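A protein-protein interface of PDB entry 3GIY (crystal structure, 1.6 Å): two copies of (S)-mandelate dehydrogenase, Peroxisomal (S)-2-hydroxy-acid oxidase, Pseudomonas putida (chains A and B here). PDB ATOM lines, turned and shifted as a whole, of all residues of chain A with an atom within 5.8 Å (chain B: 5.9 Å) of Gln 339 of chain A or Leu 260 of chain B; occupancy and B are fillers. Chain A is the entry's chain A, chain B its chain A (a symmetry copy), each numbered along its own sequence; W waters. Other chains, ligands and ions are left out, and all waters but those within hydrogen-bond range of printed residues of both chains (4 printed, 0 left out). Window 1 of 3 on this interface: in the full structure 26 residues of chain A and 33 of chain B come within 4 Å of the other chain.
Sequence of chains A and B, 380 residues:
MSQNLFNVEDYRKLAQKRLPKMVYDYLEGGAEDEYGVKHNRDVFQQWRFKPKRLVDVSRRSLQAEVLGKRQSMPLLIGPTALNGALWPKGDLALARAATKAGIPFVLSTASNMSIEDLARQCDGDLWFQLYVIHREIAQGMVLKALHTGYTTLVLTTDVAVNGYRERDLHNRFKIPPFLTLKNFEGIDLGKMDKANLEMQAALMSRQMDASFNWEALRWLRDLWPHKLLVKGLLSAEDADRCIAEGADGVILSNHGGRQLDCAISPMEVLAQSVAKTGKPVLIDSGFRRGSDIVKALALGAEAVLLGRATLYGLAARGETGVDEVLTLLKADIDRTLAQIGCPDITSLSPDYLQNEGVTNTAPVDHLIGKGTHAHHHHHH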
ATOM      1  N   ARG A  48      28.330  38.345  27.020  1.00  0.00           N
ATOM      2  CA  ARG A  48      27.676  37.156  27.546  1.00  0.00           C
ATOM      3  C   ARG A  48      26.190  37.282  27.230  1.00  0.00           C
ATOM      4  O   ARG A  48      25.702  38.372  26.929  1.00  0.00           O
ATOM      5  CB  ARG A  48      27.924  37.000  29.056  1.00  0.00           C
ATOM      6  CG  ARG A  48      29.281  36.359  29.350  1.00  0.00           C
ATOM      7  CD  ARG A  48      29.497  36.000  30.810  1.00  0.00           C
ATOM      8  NE  ARG A  48      30.657  35.116  30.939  1.00  0.00           N
ATOM      9  CZ  ARG A  48      30.617  33.785  30.840  1.00  0.00           C
ATOM     10  NH1 ARG A  48      29.466  33.150  30.622  1.00  0.00           N
ATOM     11  NH2 ARG A  48      31.742  33.084  30.931  1.00  0.00           N
ATOM     12  N   PHE A  49      25.477  36.166  27.282  1.00  0.00           N
ATOM     13  CA  PHE A  49      24.055  36.155  26.969  1.00  0.00           C
ATOM     14  C   PHE A  49      23.106  36.389  28.138  1.00  0.00           C
ATOM     15  O   PHE A  49      23.354  35.958  29.269  1.00  0.00           O
ATOM     16  CB  PHE A  49      23.674  34.821  26.324  1.00  0.00           C
ATOM     17  CG  PHE A  49      24.327  34.569  24.995  1.00  0.00           C
ATOM     18  CD1 PHE A  49      24.158  35.462  23.939  1.00  0.00           C
ATOM     19  CD2 PHE A  49      25.061  33.401  24.776  1.00  0.00           C
ATOM     20  CE1 PHE A  49      24.704  35.192  22.684  1.00  0.00           C
ATOM     21  CE2 PHE A  49      25.612  33.121  23.523  1.00  0.00           C
ATOM     22  CZ  PHE A  49      25.431  34.017  22.477  1.00  0.00           C
ATOM     23  N   PRO A  51      19.458  35.474  28.165  1.00  0.00           N
ATOM     24  CA  PRO A  51      18.320  34.779  27.559  1.00  0.00           C
ATOM     25  C   PRO A  51      16.963  35.354  27.943  1.00  0.00           C
ATOM     26  O   PRO A  51      16.787  35.880  29.042  1.00  0.00           O
ATOM     27  CB  PRO A  51      18.483  33.347  28.068  1.00  0.00           C
ATOM     28  CG  PRO A  51      19.969  33.205  28.213  1.00  0.00           C
ATOM     29  CD  PRO A  51      20.347  34.516  28.851  1.00  0.00           C
ATOM     30  N   LYS A  52      16.012  35.259  27.018  1.00  0.00           N
ATOM     31  CA  LYS A  52      14.648  35.716  27.251  1.00  0.00           C
ATOM     32  C   LYS A  52      13.856  34.429  27.431  1.00  0.00           C
ATOM     33  O   LYS A  52      13.655  33.674  26.474  1.00  0.00           O
ATOM     34  CB  LYS A  52      14.128  36.505  26.048  1.00  0.00           C
ATOM     35  CG  LYS A  52      14.898  37.796  25.778  1.00  0.00           C
ATOM     36  CD  LYS A  52      14.243  38.623  24.673  1.00  0.00           C
ATOM     37  CE  LYS A  52      15.123  39.800  24.258  1.00  0.00           C
ATOM     38  NZ  LYS A  52      15.464  40.675  25.412  1.00  0.00           N
ATOM     39  N   ARG A  53      13.438  34.175  28.669  1.00  0.00           N
ATOM     40  CA  ARG A  53      12.696  32.967  29.021  1.00  0.00           C
ATOM     41  C   ARG A  53      11.223  33.004  28.656  1.00  0.00           C
ATOM     42  O   ARG A  53      10.672  34.057  28.326  1.00  0.00           O
ATOM     43  CB  ARG A  53      12.820  32.695  30.522  1.00  0.00           C
ATOM     44  CG  ARG A  53      14.231  32.378  30.984  1.00  0.00           C
ATOM     45  CD  ARG A  53      14.774  31.136  30.297  1.00  0.00           C
ATOM     46  NE  ARG A  53      16.177  30.910  30.632  1.00  0.00           N
ATOM     47  CZ  ARG A  53      17.089  30.497  29.757  1.00  0.00           C
ATOM     48  NH1 ARG A  53      16.742  30.268  28.496  1.00  0.00           N
ATOM     49  NH2 ARG A  53      18.347  30.327  30.137  1.00  0.00           N
ATOM     50  N   VAL A  57       9.964  28.664  21.404  1.00  0.00           N
ATOM     51  CA  VAL A  57      11.036  28.444  20.440  1.00  0.00           C
ATOM     52  C   VAL A  57      10.925  27.052  19.827  1.00  0.00           C
ATOM     53  O   VAL A  57      11.923  26.457  19.427  1.00  0.00           O
ATOM     54  CB  VAL A  57      12.443  28.610  21.091  1.00  0.00           C
ATOM     55  CG1 VAL A  57      12.609  30.036  21.609  1.00  0.00           C
ATOM     56  CG2 VAL A  57      12.632  27.603  22.218  1.00  0.00           C
ATOM     57  N   ASP A 334      21.503  27.077  15.955  1.00  0.00           N
ATOM     58  CA  ASP A 334      20.105  26.760  16.237  1.00  0.00           C
ATOM     59  C   ASP A 334      19.869  26.573  17.735  1.00  0.00           C
ATOM     60  O   ASP A 334      18.924  27.127  18.310  1.00  0.00           O
ATOM     61  CB  ASP A 334      19.696  25.481  15.503  1.00  0.00           C
ATOM     62  CG  ASP A 334      18.277  25.050  15.833  1.00  0.00           C
ATOM     63  OD1 ASP A 334      17.328  25.770  15.465  1.00  0.00           O
ATOM     64  OD2 ASP A 334      18.109  23.993  16.470  1.00  0.00           O
ATOM     65  N   ARG A 335      20.738  25.781  18.350  1.00  0.00           N
ATOM     66  CA  ARG A 335      20.670  25.492  19.777  1.00  0.00           C
ATOM     67  C   ARG A 335      20.787  26.775  20.602  1.00  0.00           C
ATOM     68  O   ARG A 335      20.055  26.974  21.574  1.00  0.00           O
ATOM     69  CB  ARG A 335      21.803  24.525  20.142  1.00  0.00           C
ATOM     70  CG  ARG A 335      21.833  24.066  21.587  1.00  0.00           C
ATOM     71  CD  ARG A 335      22.995  23.100  21.814  1.00  0.00           C
ATOM     72  NE  ARG A 335      22.948  21.958  20.902  1.00  0.00           N
ATOM     73  CZ  ARG A 335      23.782  21.764  19.880  1.00  0.00           C
ATOM     74  NH1 ARG A 335      24.747  22.632  19.619  1.00  0.00           N
ATOM     75  NH2 ARG A 335      23.647  20.690  19.112  1.00  0.00           N
ATOM     76  N   THR A 336      21.714  27.643  20.204  1.00  0.00           N
ATOM     77  CA  THR A 336      21.945  28.906  20.897  1.00  0.00           C
ATOM     78  C   THR A 336      20.725  29.825  20.791  1.00  0.00           C
ATOM     79  O   THR A 336      20.310  30.428  21.782  1.00  0.00           O
ATOM     80  CB  THR A 336      23.206  29.615  20.335  1.00  0.00           C
ATOM     81  OG1 THR A 336      24.341  28.750  20.486  1.00  0.00           O
ATOM     82  CG2 THR A 336      23.476  30.907  21.083  1.00  0.00           C
ATOM     83  N   LEU A 337      20.150  29.932  19.596  1.00  0.00           N
ATOM     84  CA  LEU A 337      18.968  30.769  19.400  1.00  0.00           C
ATOM     85  C   LEU A 337      17.849  30.313  20.342  1.00  0.00           C
ATOM     86  O   LEU A 337      17.167  31.136  20.951  1.00  0.00           O
ATOM     87  CB  LEU A 337      18.486  30.696  17.942  1.00  0.00           C
ATOM     88  CG  LEU A 337      19.362  31.344  16.862  1.00  0.00           C
ATOM     89  CD1 LEU A 337      18.718  31.140  15.494  1.00  0.00           C
ATOM     90  CD2 LEU A 337      19.539  32.829  17.150  1.00  0.00           C
ATOM     91  N   ALA A 338      17.670  29.000  20.464  1.00  0.00           N
ATOM     92  CA  ALA A 338      16.640  28.444  21.332  1.00  0.00           C
ATOM     93  C   ALA A 338      16.899  28.776  22.804  1.00  0.00           C
ATOM     94  O   ALA A 338      15.990  29.188  23.529  1.00  0.00           O
ATOM     95  CB  ALA A 338      16.564  26.933  21.148  1.00  0.00           C
ATOM     96  N   GLN A 339      18.143  28.604  23.242  1.00  0.00           N
ATOM     97  CA  GLN A 339      18.496  28.862  24.628  1.00  0.00           C
ATOM     98  C   GLN A 339      18.472  30.327  25.062  1.00  0.00           C
ATOM     99  O   GLN A 339      18.379  30.612  26.257  1.00  0.00           O
ATOM    100  CB  GLN A 339      19.848  28.213  24.933  1.00  0.00           C
ATOM    101  CG  GLN A 339      19.693  26.734  25.295  1.00  0.00           C
ATOM    102  CD  GLN A 339      20.937  25.919  25.055  1.00  0.00           C
ATOM    103  OE1 GLN A 339      21.042  24.781  25.518  1.00  0.00           O
ATOM    104  NE2 GLN A 339      21.885  26.484  24.314  1.00  0.00           N
ATOM    105  N   ILE A 340      18.543  31.250  24.104  1.00  0.00           N
ATOM    106  CA  ILE A 340      18.500  32.677  24.429  1.00  0.00           C
ATOM    107  C   ILE A 340      17.101  33.245  24.172  1.00  0.00           C
ATOM    108  O   ILE A 340      16.832  34.420  24.426  1.00  0.00           O
ATOM    109  CB  ILE A 340      19.554  33.504  23.621  1.00  0.00           C
ATOM    110  CG1 ILE A 340      19.239  33.470  22.122  1.00  0.00           C
ATOM    111  CG2 ILE A 340      20.962  32.967  23.911  1.00  0.00           C
ATOM    112  CD1 ILE A 340      20.103  34.420  21.292  1.00  0.00           C
ATOM    113  N   GLY A 341      16.212  32.395  23.673  1.00  0.00           N
ATOM    114  CA  GLY A 341      14.849  32.812  23.402  1.00  0.00           C
ATOM    115  C   GLY A 341      14.634  33.654  22.154  1.00  0.00           C
ATOM    116  O   GLY A 341      13.773  34.534  22.152  1.00  0.00           O
ATOM    117  N   ALA B  31      28.286  23.043  29.843  1.00  0.00           N
ATOM    118  CA  ALA B  31      28.080  23.162  28.411  1.00  0.00           C
ATOM    119  C   ALA B  31      29.340  23.615  27.674  1.00  0.00           C
ATOM    120  O   ALA B  31      30.137  24.413  28.180  1.00  0.00           O
ATOM    121  CB  ALA B  31      26.932  24.128  28.125  1.00  0.00           C
ATOM    122  N   GLY B  36      31.438  28.876  31.275  1.00  0.00           N
ATOM    123  CA  GLY B  36      30.316  29.261  32.107  1.00  0.00           C
ATOM    124  C   GLY B  36      30.486  28.858  33.555  1.00  0.00           C
ATOM    125  O   GLY B  36      30.311  29.682  34.453  1.00  0.00           O
ATOM    126  N   ASP B 158      14.686  26.908  31.701  1.00  0.00           N
ATOM    127  CA  ASP B 158      15.895  27.006  30.882  1.00  0.00           C
ATOM    128  C   ASP B 158      16.360  25.746  30.167  1.00  0.00           C
ATOM    129  O   ASP B 158      17.554  25.596  29.879  1.00  0.00           O
ATOM    130  CB  ASP B 158      17.057  27.589  31.701  1.00  0.00           C
ATOM    131  CG  ASP B 158      17.352  26.798  32.954  1.00  0.00           C
ATOM    132  OD1 ASP B 158      16.749  25.716  33.142  1.00  0.00           O
ATOM    133  OD2 ASP B 158      18.199  27.262  33.754  1.00  0.00           O
ATOM    134  N   ALA B 160      14.554  24.463  27.213  1.00  0.00           N
ATOM    135  CA  ALA B 160      13.688  24.377  26.037  1.00  0.00           C
ATOM    136  C   ALA B 160      14.313  23.337  25.113  1.00  0.00           C
ATOM    137  O   ALA B 160      13.619  22.607  24.409  1.00  0.00           O
ATOM    138  CB  ALA B 160      13.607  25.725  25.338  1.00  0.00           C
ATOM    139  N   VAL B 161      15.642  23.296  25.130  1.00  0.00           N
ATOM    140  CA  VAL B 161      16.432  22.335  24.368  1.00  0.00           C
ATOM    141  C   VAL B 161      17.539  21.871  25.320  1.00  0.00           C
ATOM    142  O   VAL B 161      17.881  22.572  26.274  1.00  0.00           O
ATOM    143  CB  VAL B 161      17.065  22.962  23.099  1.00  0.00           C
ATOM    144  CG1 VAL B 161      15.976  23.484  22.182  1.00  0.00           C
ATOM    145  CG2 VAL B 161      18.041  24.076  23.487  1.00  0.00           C
ATOM    146  N   ASN B 162      18.081  20.684  25.075  1.00  0.00           N
ATOM    147  CA  ASN B 162      19.132  20.136  25.927  1.00  0.00           C
ATOM    148  C   ASN B 162      20.471  20.842  25.708  1.00  0.00           C
ATOM    149  O   ASN B 162      20.841  21.160  24.574  1.00  0.00           O
ATOM    150  CB  ASN B 162      19.279  18.637  25.651  1.00  0.00           C
ATOM    151  CG  ASN B 162      17.982  17.875  25.876  1.00  0.00           C
ATOM    152  OD1 ASN B 162      17.729  16.852  25.236  1.00  0.00           O
ATOM    153  ND2 ASN B 162      17.156  18.367  26.799  1.00  0.00           N
ATOM    154  N   GLY B 163      21.182  21.097  26.803  1.00  0.00           N
ATOM    155  CA  GLY B 163      22.479  21.745  26.716  1.00  0.00           C
ATOM    156  C   GLY B 163      23.499  20.855  26.023  1.00  0.00           C
ATOM    157  O   GLY B 163      23.426  19.623  26.110  1.00  0.00           O
ATOM    158  N   TYR B 164      24.448  21.475  25.325  1.00  0.00           N
ATOM    159  CA  TYR B 164      25.485  20.740  24.612  1.00  0.00           C
ATOM    160  C   TYR B 164      26.663  20.464  25.547  1.00  0.00           C
ATOM    161  O   TYR B 164      27.639  21.214  25.569  1.00  0.00           O
ATOM    162  CB  TYR B 164      25.964  21.543  23.400  1.00  0.00           C
ATOM    163  CG  TYR B 164      26.636  20.719  22.321  1.00  0.00           C
ATOM    164  CD1 TYR B 164      25.907  19.790  21.568  1.00  0.00           C
ATOM    165  CD2 TYR B 164      27.989  20.886  22.026  1.00  0.00           C
ATOM    166  CE1 TYR B 164      26.510  19.055  20.544  1.00  0.00           C
ATOM    167  CE2 TYR B 164      28.607  20.153  21.003  1.00  0.00           C
ATOM    168  CZ  TYR B 164      27.859  19.244  20.264  1.00  0.00           C
ATOM    169  OH  TYR B 164      28.450  18.544  19.232  1.00  0.00           O
ATOM    170  N   ASN B 254      21.521  29.892  35.897  1.00  0.00           N
ATOM    171  CA  ASN B 254      21.961  29.539  34.552  1.00  0.00           C
ATOM    172  C   ASN B 254      22.172  28.021  34.529  1.00  0.00           C
ATOM    173  O   ASN B 254      22.951  27.484  33.742  1.00  0.00           O
ATOM    174  CB  ASN B 254      23.221  30.319  34.082  1.00  0.00           C
ATOM    175  CG  ASN B 254      24.442  30.109  34.960  1.00  0.00           C
ATOM    176  OD1 ASN B 254      24.652  29.036  35.520  1.00  0.00           O
ATOM    177  ND2 ASN B 254      25.279  31.138  35.050  1.00  0.00           N
ATOM    178  N   GLY B 257      25.706  26.421  34.782  1.00  0.00           N
ATOM    179  CA  GLY B 257      26.522  26.444  33.578  1.00  0.00           C
ATOM    180  C   GLY B 257      26.376  25.217  32.691  1.00  0.00           C
ATOM    181  O   GLY B 257      27.253  24.934  31.874  1.00  0.00           O
ATOM    182  N   ARG B 258      25.258  24.502  32.824  1.00  0.00           N
ATOM    183  CA  ARG B 258      25.034  23.278  32.053  1.00  0.00           C
ATOM    184  C   ARG B 258      24.192  23.436  30.795  1.00  0.00           C
ATOM    185  O   ARG B 258      24.066  22.493  30.014  1.00  0.00           O
ATOM    186  CB  ARG B 258      24.386  22.224  32.952  1.00  0.00           C
ATOM    187  CG  ARG B 258      25.256  21.799  34.127  1.00  0.00           C
ATOM    188  CD  ARG B 258      24.432  21.109  35.199  1.00  0.00           C
ATOM    189  NE  ARG B 258      23.933  19.789  34.809  1.00  0.00           N
ATOM    190  CZ  ARG B 258      24.688  18.697  34.724  1.00  0.00           C
ATOM    191  NH1 ARG B 258      25.989  18.766  34.990  1.00  0.00           N
ATOM    192  NH2 ARG B 258      24.135  17.527  34.416  1.00  0.00           N
ATOM    193  N   GLN B 259      23.626  24.620  30.591  1.00  0.00           N
ATOM    194  CA  GLN B 259      22.775  24.856  29.432  1.00  0.00           C
ATOM    195  C   GLN B 259      23.357  25.745  28.330  1.00  0.00           C
ATOM    196  O   GLN B 259      23.291  25.397  27.148  1.00  0.00           O
ATOM    197  CB  GLN B 259      21.428  25.418  29.910  1.00  0.00           C
ATOM    198  CG  GLN B 259      20.554  24.380  30.611  1.00  0.00           C
ATOM    199  CD  GLN B 259      20.122  23.277  29.661  1.00  0.00           C
ATOM    200  OE1 GLN B 259      19.341  23.510  28.738  1.00  0.00           O
ATOM    201  NE2 GLN B 259      20.640  22.075  29.872  1.00  0.00           N
ATOM    202  N   LEU B 260      23.920  26.888  28.715  1.00  0.00           N
ATOM    203  CA  LEU B 260      24.484  27.842  27.762  1.00  0.00           C
ATOM    204  C   LEU B 260      25.815  28.333  28.329  1.00  0.00           C
ATOM    205  O   LEU B 260      25.853  29.082  29.300  1.00  0.00           O
ATOM    206  CB  LEU B 260      23.505  29.011  27.577  1.00  0.00           C
ATOM    207  CG  LEU B 260      23.843  30.150  26.611  1.00  0.00           C
ATOM    208  CD1 LEU B 260      23.912  29.623  25.187  1.00  0.00           C
ATOM    209  CD2 LEU B 260      22.785  31.236  26.719  1.00  0.00           C
ATOM    210  N   ASP B 261      26.912  27.918  27.714  1.00  0.00           N
ATOM    211  CA  ASP B 261      28.227  28.293  28.214  1.00  0.00           C
ATOM    212  C   ASP B 261      28.491  29.795  28.404  1.00  0.00           C
ATOM    213  O   ASP B 261      29.143  30.189  29.375  1.00  0.00           O
ATOM    214  CB  ASP B 261      29.313  27.679  27.320  1.00  0.00           C
ATOM    215  CG  ASP B 261      30.645  27.547  28.036  1.00  0.00           C
ATOM    216  OD1 ASP B 261      30.639  27.189  29.234  1.00  0.00           O
ATOM    217  OD2 ASP B 261      31.700  27.787  27.408  1.00  0.00           O
ATOM    218  N   CYS B 262      27.979  30.629  27.499  1.00  0.00           N
ATOM    219  CA  CYS B 262      28.213  32.074  27.571  1.00  0.00           C
ATOM    220  C   CYS B 262      27.137  32.888  28.269  1.00  0.00           C
ATOM    221  O   CYS B 262      27.087  34.110  28.126  1.00  0.00           O
ATOM    222  CB  CYS B 262      28.442  32.643  26.169  1.00  0.00           C
ATOM    223  SG  CYS B 262      29.920  31.995  25.341  1.00  0.00           S
ATOM    224  N   ALA B 263      26.276  32.217  29.021  1.00  0.00           N
ATOM    225  CA  ALA B 263      25.228  32.916  29.750  1.00  0.00           C
ATOM    226  C   ALA B 263      25.882  33.720  30.866  1.00  0.00           C
ATOM    227  O   ALA B 263      26.971  33.378  31.339  1.00  0.00           O
ATOM    228  CB  ALA B 263      24.244  31.914  30.346  1.00  0.00           C
HETATM  229  O   HOH W   1      27.972  31.258  33.140  1.00  0.00           O
HETATM  230  O   HOH W   2      20.333  20.167  22.028  1.00  0.00           O
HETATM  231  O   HOH W   3      19.391  29.658  32.754  1.00  0.00           O
HETATM  232  O   HOH W   4      24.486  24.349  25.043  1.00  0.00           O
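No position is printed for both chains.
Of the 17 pairs that touch across the chains among the printed residues, none has its exchanged pair printed and touching as well.
Water W4 lies within hydrogen-bond range of the backbone carbonyl oxygen of Gln 259 of chain B (2.6 Å), the backbone NH of Tyr 164 of chain B (2.9 Å) and the side-chain amide nitrogen of Gln 339 of chain A (3.4 Å).
Water W2 bridges O of Asn 162 of chain B (2.8 Å) and NE of Arg 335 of chain A (3.4 Å).
Water W3 lies within hydrogen-bond range of the side-chain carboxylate of Asp 158 of chain B (2.9 Å) and the guanidinium group of Arg 53 of chain A (2.9 Å).
Water W1 lies within hydrogen-bond range of O of Ala 263 of chain B, O of Gly 36 of chain B, ND2 of Asn 254 of chain B and NH1 of Arg 48 of chain A.
The backbone NH (N) of Lys 52 of chain A is in hydrogen-bond range of the backbone carbonyl oxygen (O) of Ile 340 of chain A, 2.8 Å away.
The backbone carbonyl oxygen of Gln 339 of chain A is in hydrogen-bond range of the guanidinium group of Arg 53 of chain A (2.8 Å).
The side-chain amide nitrogen of Gln 339 of chain A sits at hydrogen-bond distance from the backbone carbonyl oxygen of Arg 335 of chain A, 3.3 Å away.
The backbone NH of Gly 36 of chain B is in hydrogen-bond range of the side-chain carboxylate of Asp 261 of chain B (2.8 Å).
OE1 of Gln 259 of chain B lies close to O of Asp 158 of chain B.
The side-chain amide oxygen of Gln 259 of chain B sits close to the backbone carbonyl oxygen of Val 161 of chain B, at 3.0 Å.
Of chain B, only Val 161, Asn 162, Gly 163, Gln 259 and Leu 260 come within 4 Å of Gln 339 of chain A.
Leu 260 of chain B touches four residues of chain A.
Of the printed residues of chain B, Val 57 of chain A touches Ala 160.
Printed residues of chain A within 4 Å of Asp 261 of chain B: Arg 48 (3.2 Å).
Of the printed residues of chain B, Ile 340 of chain A touches Leu 260 (3.8 Å).
Of the 14 printed residues of chain A, 9 touch a printed residue of chain B.
NH1 of Arg 48 of chain A is in hydrogen-bond range of O of Asp 261 of chain B, at 3.2 Å.
The backbone carbonyl oxygen (O) of Ala 263 of chain B lies within hydrogen-bond range of the guanidinium group (NH1) of Arg 48 of chain A.
The backbone NH of Phe 49 of chain A sits at hydrogen-bond distance from the backbone carbonyl oxygen of Cys 262 of chain B (2.7 Å).
The side-chain amide oxygen (OE1) of Gln 339 of chain A sits close to the backbone carbonyl oxygen (O) of Gln 259 of chain B (2.8 Å).
Among the printed residues, pairs that only touch across the chains: Arg 48 of chain A with Cys 262 of chain B (3.1 Å), Arg 335 of chain A with Tyr 164 of chain B (3.4 Å), Arg 53 of chain A with Asp 158 of chain B (3.4 Å), Gln 339 of chain A with Gly 163 of chain B (3.6 Å), Phe 49 of chain A with Ala 263 of chain B (3.6 Å), Gln 339 of chain A with Val 161 of chain B (3.6 Å), Ala 338 of chain A with Val 161 of chain B (3.6 Å), Phe 49 of chain A with Leu 260 of chain B (3.7 Å), Pro 51 of chain A with Leu 260 of chain B (3.7 Å), Gln 339 of chain A with Asn 162 of chain B (3.7 Å), Ile 340 of chain A with Leu 260 of chain B (3.8 Å), Val 57 of chain A with Ala 160 of chain B (3.8 Å) and Gln 339 of chain A with Leu 260 of chain B (3.8 Å).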
